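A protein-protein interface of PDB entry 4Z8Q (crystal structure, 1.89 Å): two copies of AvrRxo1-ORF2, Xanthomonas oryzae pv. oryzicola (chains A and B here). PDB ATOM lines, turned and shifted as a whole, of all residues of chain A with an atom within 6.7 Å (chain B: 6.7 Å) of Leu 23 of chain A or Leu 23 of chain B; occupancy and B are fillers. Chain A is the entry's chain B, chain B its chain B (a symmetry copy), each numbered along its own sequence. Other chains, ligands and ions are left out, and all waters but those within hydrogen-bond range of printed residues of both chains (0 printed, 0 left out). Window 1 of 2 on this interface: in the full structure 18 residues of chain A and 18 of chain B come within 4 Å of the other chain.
The side-chain hydroxyl of Ser 26 of chain B sits at hydrogen-bond distance from the guanidinium group of Arg 19 of chain A, at 2.8 Å.
The side-chain carboxylate (OD1) of Asp 27 of chain B is in salt-bridge range of the guanidinium group (NH1) of Arg 19 of chain A (2.9 Å).
OG of Ser 26 of chain A lies within hydrogen-bond range of NH1 of Arg 19 of chain B, at 2.8 Å.
NH1 of Arg 19 of chain B is in salt-bridge range of OD1 of Asp 27 of chain A (2.9 Å).
Among the printed residues, merely in contact across the chains: Arg 19 of chain A with Leu 23 of chain B (3.6 Å), Ala 22 of chain A with Ala 22 of chain B (3.9 Å), Leu 23 of chain A with Arg 19 of chain B (3.6 Å) and Leu 23 of chain A with Leu 23 of chain B (3.5 Å).
Of chain A, only Arg 19 (3.6 Å) and Leu 23 (3.5 Å) come within 4 Å of Leu 23 of chain B.
Printed residues of chain A within 4 Å of Ser 26 of chain B: Arg 19.
Printed residues of chain B within 4 Å of Ser 26 of chain A: Arg 19 (2.8 Å).
Of the printed residues of chain B, Asp 27 of chain A touches Arg 19.
Of the printed residues of chain A, Arg 19 of chain B touches Leu 23 (3.6 Å), Ser 26 (2.8 Å) and Asp 27 (2.9 Å).
Printed residues of chain A within 4 Å of Asp 27 of chain B: Arg 19.
The nearest residue of chain A that does not touch Leu 23 of chain B is Ala 22 of chain A (6.2 Å).
The nearest printed residue of chain A that does not touch Asp 27 of chain B is Leu 23 of chain A (8.3 Å).
Of the 12 printed residues of chain A, 5 touch a printed residue of chain B.
Among the printed residues, 8 pairs touch across the chains.
Among the printed residues, Asp or Glu carboxylates within 4 Å of a Lys or Arg side-chain nitrogen of the other chain: Arg 19 of chain A with Asp 27 of chain B and Asp 27 of chain A with Arg 19 of chain B.
Arg 19 of chain A touches Ser 26 of chain B, and with the chains exchanged Ser 26 of chain A touches Arg 19 of chain B.
Arg 19 of chain A touches Asp 27 of chain B, and with the chains exchanged Asp 27 of chain A touches Arg 19 of chain B.
Ala 22 of chain A touches its own counterpart, Ala 22 of chain B.
Leu 23 of chain B touches its own counterpart, Leu 23 of chain A.
Positions printed for both chains: 18, 19, 20, 21, 22, 23, 24, 25, 26, 27, 28 and 72.
Of the 8 pairs that touch across the chains among the printed residues, 8 have their exchanged pair printed and touching as well.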
ATOM      1  N   GLU A  18      -2.325  19.458 -27.508  1.00  0.00           N
ATOM      2  CA  GLU A  18      -2.282  17.998 -27.426  1.00  0.00           C
ATOM      3  C   GLU A  18      -3.609  17.390 -27.816  1.00  0.00           C
ATOM      4  O   GLU A  18      -3.656  16.396 -28.526  1.00  0.00           O
ATOM      5  CB  GLU A  18      -1.954  17.551 -25.999  1.00  0.00           C
ATOM      6  CG  GLU A  18      -0.589  17.955 -25.521  1.00  0.00           C
ATOM      7  CD  GLU A  18      -0.355  17.576 -24.073  1.00  0.00           C
ATOM      8  OE1 GLU A  18      -1.167  16.790 -23.520  1.00  0.00           O
ATOM      9  OE2 GLU A  18       0.642  18.065 -23.494  1.00  0.00           O
ATOM     10  N   ARG A  19      -4.686  17.986 -27.327  1.00  0.00           N
ATOM     11  CA  ARG A  19      -6.029  17.546 -27.675  1.00  0.00           C
ATOM     12  C   ARG A  19      -6.234  17.622 -29.182  1.00  0.00           C
ATOM     13  O   ARG A  19      -6.660  16.650 -29.805  1.00  0.00           O
ATOM     14  CB  ARG A  19      -7.055  18.434 -26.977  1.00  0.00           C
ATOM     15  CG  ARG A  19      -8.501  18.235 -27.427  1.00  0.00           C
ATOM     16  CD  ARG A  19      -9.369  19.373 -26.905  1.00  0.00           C
ATOM     17  NE  ARG A  19     -10.802  19.118 -27.070  1.00  0.00           N
ATOM     18  CZ  ARG A  19     -11.535  18.421 -26.200  1.00  0.00           C
ATOM     19  NH1 ARG A  19     -10.975  17.907 -25.103  1.00  0.00           N
ATOM     20  NH2 ARG A  19     -12.827  18.244 -26.417  1.00  0.00           N
ATOM     21  N   ASN A  20      -5.914  18.772 -29.774  1.00  0.00           N
ATOM     22  CA  ASN A  20      -6.173  18.967 -31.197  1.00  0.00           C
ATOM     23  C   ASN A  20      -5.289  18.079 -32.053  1.00  0.00           C
ATOM     24  O   ASN A  20      -5.707  17.626 -33.108  1.00  0.00           O
ATOM     25  CB  ASN A  20      -6.022  20.447 -31.588  1.00  0.00           C
ATOM     26  CG  ASN A  20      -7.151  21.304 -31.045  1.00  0.00           C
ATOM     27  OD1 ASN A  20      -8.235  20.793 -30.731  1.00  0.00           O
ATOM     28  ND2 ASN A  20      -6.913  22.610 -30.940  1.00  0.00           N
ATOM     29  N   LYS A  21      -4.067  17.828 -31.599  1.00  0.00           N
ATOM     30  CA  LYS A  21      -3.164  16.917 -32.301  1.00  0.00           C
ATOM     31  C   LYS A  21      -3.700  15.489 -32.253  1.00  0.00           C
ATOM     32  O   LYS A  21      -3.623  14.735 -33.235  1.00  0.00           O
ATOM     33  CB  LYS A  21      -1.763  16.955 -31.668  1.00  0.00           C
ATOM     34  CG  LYS A  21      -0.788  15.931 -32.258  1.00  0.00           C
ATOM     35  CD  LYS A  21       0.606  16.062 -31.635  1.00  0.00           C
ATOM     36  CE  LYS A  21       1.701  15.577 -32.586  1.00  0.00           C
ATOM     37  NZ  LYS A  21       3.074  15.841 -32.049  1.00  0.00           N
ATOM     38  N   ALA A  22      -4.238  15.106 -31.103  1.00  0.00           N
ATOM     39  CA  ALA A  22      -4.857  13.794 -31.002  1.00  0.00           C
ATOM     40  C   ALA A  22      -6.104  13.700 -31.881  1.00  0.00           C
ATOM     41  O   ALA A  22      -6.345  12.669 -32.504  1.00  0.00           O
ATOM     42  CB  ALA A  22      -5.170  13.460 -29.557  1.00  0.00           C
ATOM     43  N   LEU A  23      -6.899  14.766 -31.945  1.00  0.00           N
ATOM     44  CA  LEU A  23      -8.072  14.756 -32.816  1.00  0.00           C
ATOM     45  C   LEU A  23      -7.664  14.743 -34.287  1.00  0.00           C
ATOM     46  O   LEU A  23      -8.269  14.038 -35.093  1.00  0.00           O
ATOM     47  CB  LEU A  23      -8.987  15.950 -32.550  1.00  0.00           C
ATOM     48  CG  LEU A  23      -9.733  15.985 -31.220  1.00  0.00           C
ATOM     49  CD1 LEU A  23     -10.216  17.398 -30.938  1.00  0.00           C
ATOM     50  CD2 LEU A  23     -10.920  15.030 -31.284  1.00  0.00           C
ATOM     51  N   HIS A  24      -6.637  15.520 -34.623  1.00  0.00           N
ATOM     52  CA  HIS A  24      -6.103  15.594 -35.984  1.00  0.00           C
ATOM     53  C   HIS A  24      -5.717  14.184 -36.474  1.00  0.00           C
ATOM     54  O   HIS A  24      -6.169  13.720 -37.527  1.00  0.00           O
ATOM     55  CB  HIS A  24      -4.879  16.519 -35.966  1.00  0.00           C
ATOM     56  CG  HIS A  24      -4.448  17.027 -37.310  1.00  0.00           C
ATOM     57  ND1 HIS A  24      -5.235  17.858 -38.082  1.00  0.00           N
ATOM     58  CD2 HIS A  24      -3.285  16.874 -37.987  1.00  0.00           C
ATOM     59  CE1 HIS A  24      -4.584  18.168 -39.191  1.00  0.00           C
ATOM     60  NE2 HIS A  24      -3.400  17.582 -39.160  1.00  0.00           N
ATOM     61  N   ALA A  25      -4.876  13.502 -35.706  1.00  0.00           N
ATOM     62  CA  ALA A  25      -4.452  12.155 -36.061  1.00  0.00           C
ATOM     63  C   ALA A  25      -5.641  11.190 -36.118  1.00  0.00           C
ATOM     64  O   ALA A  25      -5.761  10.406 -37.062  1.00  0.00           O
ATOM     65  CB  ALA A  25      -3.401  11.649 -35.078  1.00  0.00           C
ATOM     66  N   SER A  26      -6.523  11.262 -35.118  1.00  0.00           N
ATOM     67  CA  SER A  26      -7.713  10.409 -35.070  1.00  0.00           C
ATOM     68  C   SER A  26      -8.661  10.563 -36.259  1.00  0.00           C
ATOM     69  O   SER A  26      -9.130   9.567 -36.823  1.00  0.00           O
ATOM     70  CB  SER A  26      -8.487  10.634 -33.769  1.00  0.00           C
ATOM     71  OG  SER A  26      -9.769  10.042 -33.859  1.00  0.00           O
ATOM     72  N   ASP A  27      -8.957  11.798 -36.645  1.00  0.00           N
ATOM     73  CA  ASP A  27      -9.808  12.020 -37.806  1.00  0.00           C
ATOM     74  C   ASP A  27      -9.281  11.281 -39.042  1.00  0.00           C
ATOM     75  O   ASP A  27     -10.056  10.740 -39.835  1.00  0.00           O
ATOM     76  CB  ASP A  27      -9.893  13.510 -38.139  1.00  0.00           C
ATOM     77  CG  ASP A  27     -10.739  14.290 -37.159  1.00  0.00           C
ATOM     78  OD1 ASP A  27     -11.579  13.684 -36.473  1.00  0.00           O
ATOM     79  OD2 ASP A  27     -10.578  15.524 -37.107  1.00  0.00           O
ATOM     80  N   LEU A  28      -7.969  11.280 -39.225  1.00  0.00           N
ATOM     81  CA  LEU A  28      -7.403  10.622 -40.411  1.00  0.00           C
ATOM     82  C   LEU A  28      -7.420   9.098 -40.257  1.00  0.00           C
ATOM     83  O   LEU A  28      -7.788   8.385 -41.192  1.00  0.00           O
ATOM     84  CB  LEU A  28      -5.994  11.121 -40.716  1.00  0.00           C
ATOM     85  CG  LEU A  28      -5.265  10.426 -41.873  1.00  0.00           C
ATOM     86  CD1 LEU A  28      -5.987  10.597 -43.201  1.00  0.00           C
ATOM     87  CD2 LEU A  28      -3.836  10.940 -41.987  1.00  0.00           C
ATOM     88  N   ARG A  72      -4.797  14.180 -46.632  1.00  0.00           N
ATOM     89  CA  ARG A  72      -5.720  14.428 -45.545  1.00  0.00           C
ATOM     90  C   ARG A  72      -7.052  15.054 -45.992  1.00  0.00           C
ATOM     91  O   ARG A  72      -8.098  14.719 -45.532  1.00  0.00           O
ATOM     92  CB  ARG A  72      -5.031  15.248 -44.474  1.00  0.00           C
ATOM     93  CG  ARG A  72      -5.939  15.678 -43.403  1.00  0.00           C
ATOM     94  CD  ARG A  72      -5.311  16.553 -42.407  1.00  0.00           C
ATOM     95  NE  ARG A  72      -4.496  15.731 -41.580  1.00  0.00           N
ATOM     96  CZ  ARG A  72      -4.931  15.123 -40.486  1.00  0.00           C
ATOM     97  NH1 ARG A  72      -4.102  14.386 -39.867  1.00  0.00           N
ATOM     98  NH2 ARG A  72      -6.159  15.293 -40.016  1.00  0.00           N
ATOM     99  N   GLU B  18      -9.258   5.082 -28.707  1.00  0.00           N
ATOM    100  CA  GLU B  18      -8.090   5.932 -28.472  1.00  0.00           C
ATOM    101  C   GLU B  18      -8.461   7.396 -28.527  1.00  0.00           C
ATOM    102  O   GLU B  18      -8.008   8.186 -27.711  1.00  0.00           O
ATOM    103  CB  GLU B  18      -7.015   5.672 -29.531  1.00  0.00           C
ATOM    104  CG  GLU B  18      -6.436   4.287 -29.498  1.00  0.00           C
ATOM    105  CD  GLU B  18      -5.453   4.053 -30.627  1.00  0.00           C
ATOM    106  OE1 GLU B  18      -5.050   5.045 -31.287  1.00  0.00           O
ATOM    107  OE2 GLU B  18      -5.085   2.876 -30.848  1.00  0.00           O
ATOM    108  N   ARG B  19      -9.272   7.752 -29.512  1.00  0.00           N
ATOM    109  CA  ARG B  19      -9.761   9.116 -29.645  1.00  0.00           C
ATOM    110  C   ARG B  19     -10.523   9.527 -28.391  1.00  0.00           C
ATOM    111  O   ARG B  19     -10.246  10.575 -27.808  1.00  0.00           O
ATOM    112  CB  ARG B  19     -10.686   9.212 -30.855  1.00  0.00           C
ATOM    113  CG  ARG B  19     -11.453  10.526 -30.986  1.00  0.00           C
ATOM    114  CD  ARG B  19     -12.558  10.382 -32.025  1.00  0.00           C
ATOM    115  NE  ARG B  19     -13.162  11.665 -32.396  1.00  0.00           N
ATOM    116  CZ  ARG B  19     -12.661  12.478 -33.326  1.00  0.00           C
ATOM    117  NH1 ARG B  19     -11.548  12.148 -33.984  1.00  0.00           N
ATOM    118  NH2 ARG B  19     -13.273  13.615 -33.609  1.00  0.00           N
ATOM    119  N   ASN B  20     -11.469   8.693 -27.964  1.00  0.00           N
ATOM    120  CA  ASN B  20     -12.316   9.055 -26.831  1.00  0.00           C
ATOM    121  C   ASN B  20     -11.527   9.099 -25.536  1.00  0.00           C
ATOM    122  O   ASN B  20     -11.813   9.908 -24.666  1.00  0.00           O
ATOM    123  CB  ASN B  20     -13.521   8.106 -26.717  1.00  0.00           C
ATOM    124  CG  ASN B  20     -14.536   8.331 -27.823  1.00  0.00           C
ATOM    125  OD1 ASN B  20     -14.578   9.409 -28.432  1.00  0.00           O
ATOM    126  ND2 ASN B  20     -15.369   7.324 -28.083  1.00  0.00           N
ATOM    127  N   LYS B  21     -10.529   8.232 -25.408  1.00  0.00           N
ATOM    128  CA  LYS B  21      -9.651   8.245 -24.238  1.00  0.00           C
ATOM    129  C   LYS B  21      -8.818   9.523 -24.208  1.00  0.00           C
ATOM    130  O   LYS B  21      -8.594  10.125 -23.147  1.00  0.00           O
ATOM    131  CB  LYS B  21      -8.712   7.027 -24.257  1.00  0.00           C
ATOM    132  CG  LYS B  21      -7.668   7.033 -23.137  1.00  0.00           C
ATOM    133  CD  LYS B  21      -6.807   5.766 -23.169  1.00  0.00           C
ATOM    134  CE  LYS B  21      -6.254   5.420 -21.784  1.00  0.00           C
ATOM    135  NZ  LYS B  21      -5.540   4.103 -21.774  1.00  0.00           N
ATOM    136  N   ALA B  22      -8.346   9.939 -25.376  1.00  0.00           N
ATOM    137  CA  ALA B  22      -7.623  11.198 -25.449  1.00  0.00           C
ATOM    138  C   ALA B  22      -8.538  12.383 -25.138  1.00  0.00           C
ATOM    139  O   ALA B  22      -8.123  13.325 -24.469  1.00  0.00           O
ATOM    140  CB  ALA B  22      -6.955  11.354 -26.801  1.00  0.00           C
ATOM    141  N   LEU B  23      -9.783  12.345 -25.609  1.00  0.00           N
ATOM    142  CA  LEU B  23     -10.721  13.419 -25.292  1.00  0.00           C
ATOM    143  C   LEU B  23     -11.086  13.410 -23.810  1.00  0.00           C
ATOM    144  O   LEU B  23     -11.178  14.467 -23.187  1.00  0.00           O
ATOM    145  CB  LEU B  23     -11.994  13.328 -26.132  1.00  0.00           C
ATOM    146  CG  LEU B  23     -11.874  13.609 -27.626  1.00  0.00           C
ATOM    147  CD1 LEU B  23     -13.086  13.050 -28.354  1.00  0.00           C
ATOM    148  CD2 LEU B  23     -11.779  15.114 -27.849  1.00  0.00           C
ATOM    149  N   HIS B  24     -11.285  12.217 -23.256  1.00  0.00           N
ATOM    150  CA  HIS B  24     -11.609  12.036 -21.840  1.00  0.00           C
ATOM    151  C   HIS B  24     -10.531  12.708 -20.966  1.00  0.00           C
ATOM    152  O   HIS B  24     -10.826  13.549 -20.110  1.00  0.00           O
ATOM    153  CB  HIS B  24     -11.680  10.530 -21.556  1.00  0.00           C
ATOM    154  CG  HIS B  24     -12.380  10.158 -20.283  1.00  0.00           C
ATOM    155  ND1 HIS B  24     -13.722  10.400 -20.069  1.00  0.00           N
ATOM    156  CD2 HIS B  24     -11.936   9.501 -19.184  1.00  0.00           C
ATOM    157  CE1 HIS B  24     -14.065   9.935 -18.879  1.00  0.00           C
ATOM    158  NE2 HIS B  24     -13.000   9.387 -18.320  1.00  0.00           N
ATOM    159  N   ALA B  25      -9.276  12.334 -21.184  1.00  0.00           N
ATOM    160  CA  ALA B  25      -8.173  12.912 -20.428  1.00  0.00           C
ATOM    161  C   ALA B  25      -8.070  14.423 -20.656  1.00  0.00           C
ATOM    162  O   ALA B  25      -7.908  15.186 -19.701  1.00  0.00           O
ATOM    163  CB  ALA B  25      -6.860  12.225 -20.791  1.00  0.00           C
ATOM    164  N   SER B  26      -8.179  14.851 -21.916  1.00  0.00           N
ATOM    165  CA  SER B  26      -8.119  16.274 -22.261  1.00  0.00           C
ATOM    166  C   SER B  26      -9.193  17.139 -21.602  1.00  0.00           C
ATOM    167  O   SER B  26      -8.897  18.222 -21.084  1.00  0.00           O
ATOM    168  CB  SER B  26      -8.169  16.464 -23.779  1.00  0.00           C
ATOM    169  OG  SER B  26      -8.411  17.824 -24.088  1.00  0.00           O
ATOM    170  N   ASP B  27     -10.438  16.681 -21.621  1.00  0.00           N
ATOM    171  CA  ASP B  27     -11.503  17.425 -20.963  1.00  0.00           C
ATOM    172  C   ASP B  27     -11.161  17.726 -19.498  1.00  0.00           C
ATOM    173  O   ASP B  27     -11.460  18.809 -18.987  1.00  0.00           O
ATOM    174  CB  ASP B  27     -12.815  16.638 -20.996  1.00  0.00           C
ATOM    175  CG  ASP B  27     -13.453  16.608 -22.366  1.00  0.00           C
ATOM    176  OD1 ASP B  27     -13.149  17.483 -23.192  1.00  0.00           O
ATOM    177  OD2 ASP B  27     -14.291  15.714 -22.596  1.00  0.00           O
ATOM    178  N   LEU B  28     -10.562  16.763 -18.814  1.00  0.00           N
ATOM    179  CA  LEU B  28     -10.241  16.974 -17.395  1.00  0.00           C
ATOM    180  C   LEU B  28      -9.027  17.895 -17.235  1.00  0.00           C
ATOM    181  O   LEU B  28      -9.043  18.801 -16.401  1.00  0.00           O
ATOM    182  CB  LEU B  28     -10.021  15.654 -16.663  1.00  0.00           C
ATOM    183  CG  LEU B  28      -9.578  15.758 -15.198  1.00  0.00           C
ATOM    184  CD1 LEU B  28     -10.605  16.469 -14.329  1.00  0.00           C
ATOM    185  CD2 LEU B  28      -9.284  14.375 -14.632  1.00  0.00           C
ATOM    186  N   ARG B  72     -14.087  14.041 -11.500  1.00  0.00           N
ATOM    187  CA  ARG B  72     -14.317  14.375 -12.889  1.00  0.00           C
ATOM    188  C   ARG B  72     -15.653  15.093 -13.143  1.00  0.00           C
ATOM    189  O   ARG B  72     -15.750  16.005 -13.902  1.00  0.00           O
ATOM    190  CB  ARG B  72     -14.165  13.131 -13.740  1.00  0.00           C
ATOM    191  CG  ARG B  72     -14.532  13.343 -15.145  1.00  0.00           C
ATOM    192  CD  ARG B  72     -14.482  12.126 -15.964  1.00  0.00           C
ATOM    193  NE  ARG B  72     -13.111  11.846 -16.217  1.00  0.00           N
ATOM    194  CZ  ARG B  72     -12.436  12.334 -17.248  1.00  0.00           C
ATOM    195  NH1 ARG B  72     -11.205  12.032 -17.326  1.00  0.00           N
ATOM    196  NH2 ARG B  72     -13.008  13.071 -18.190  1.00  0.00           N
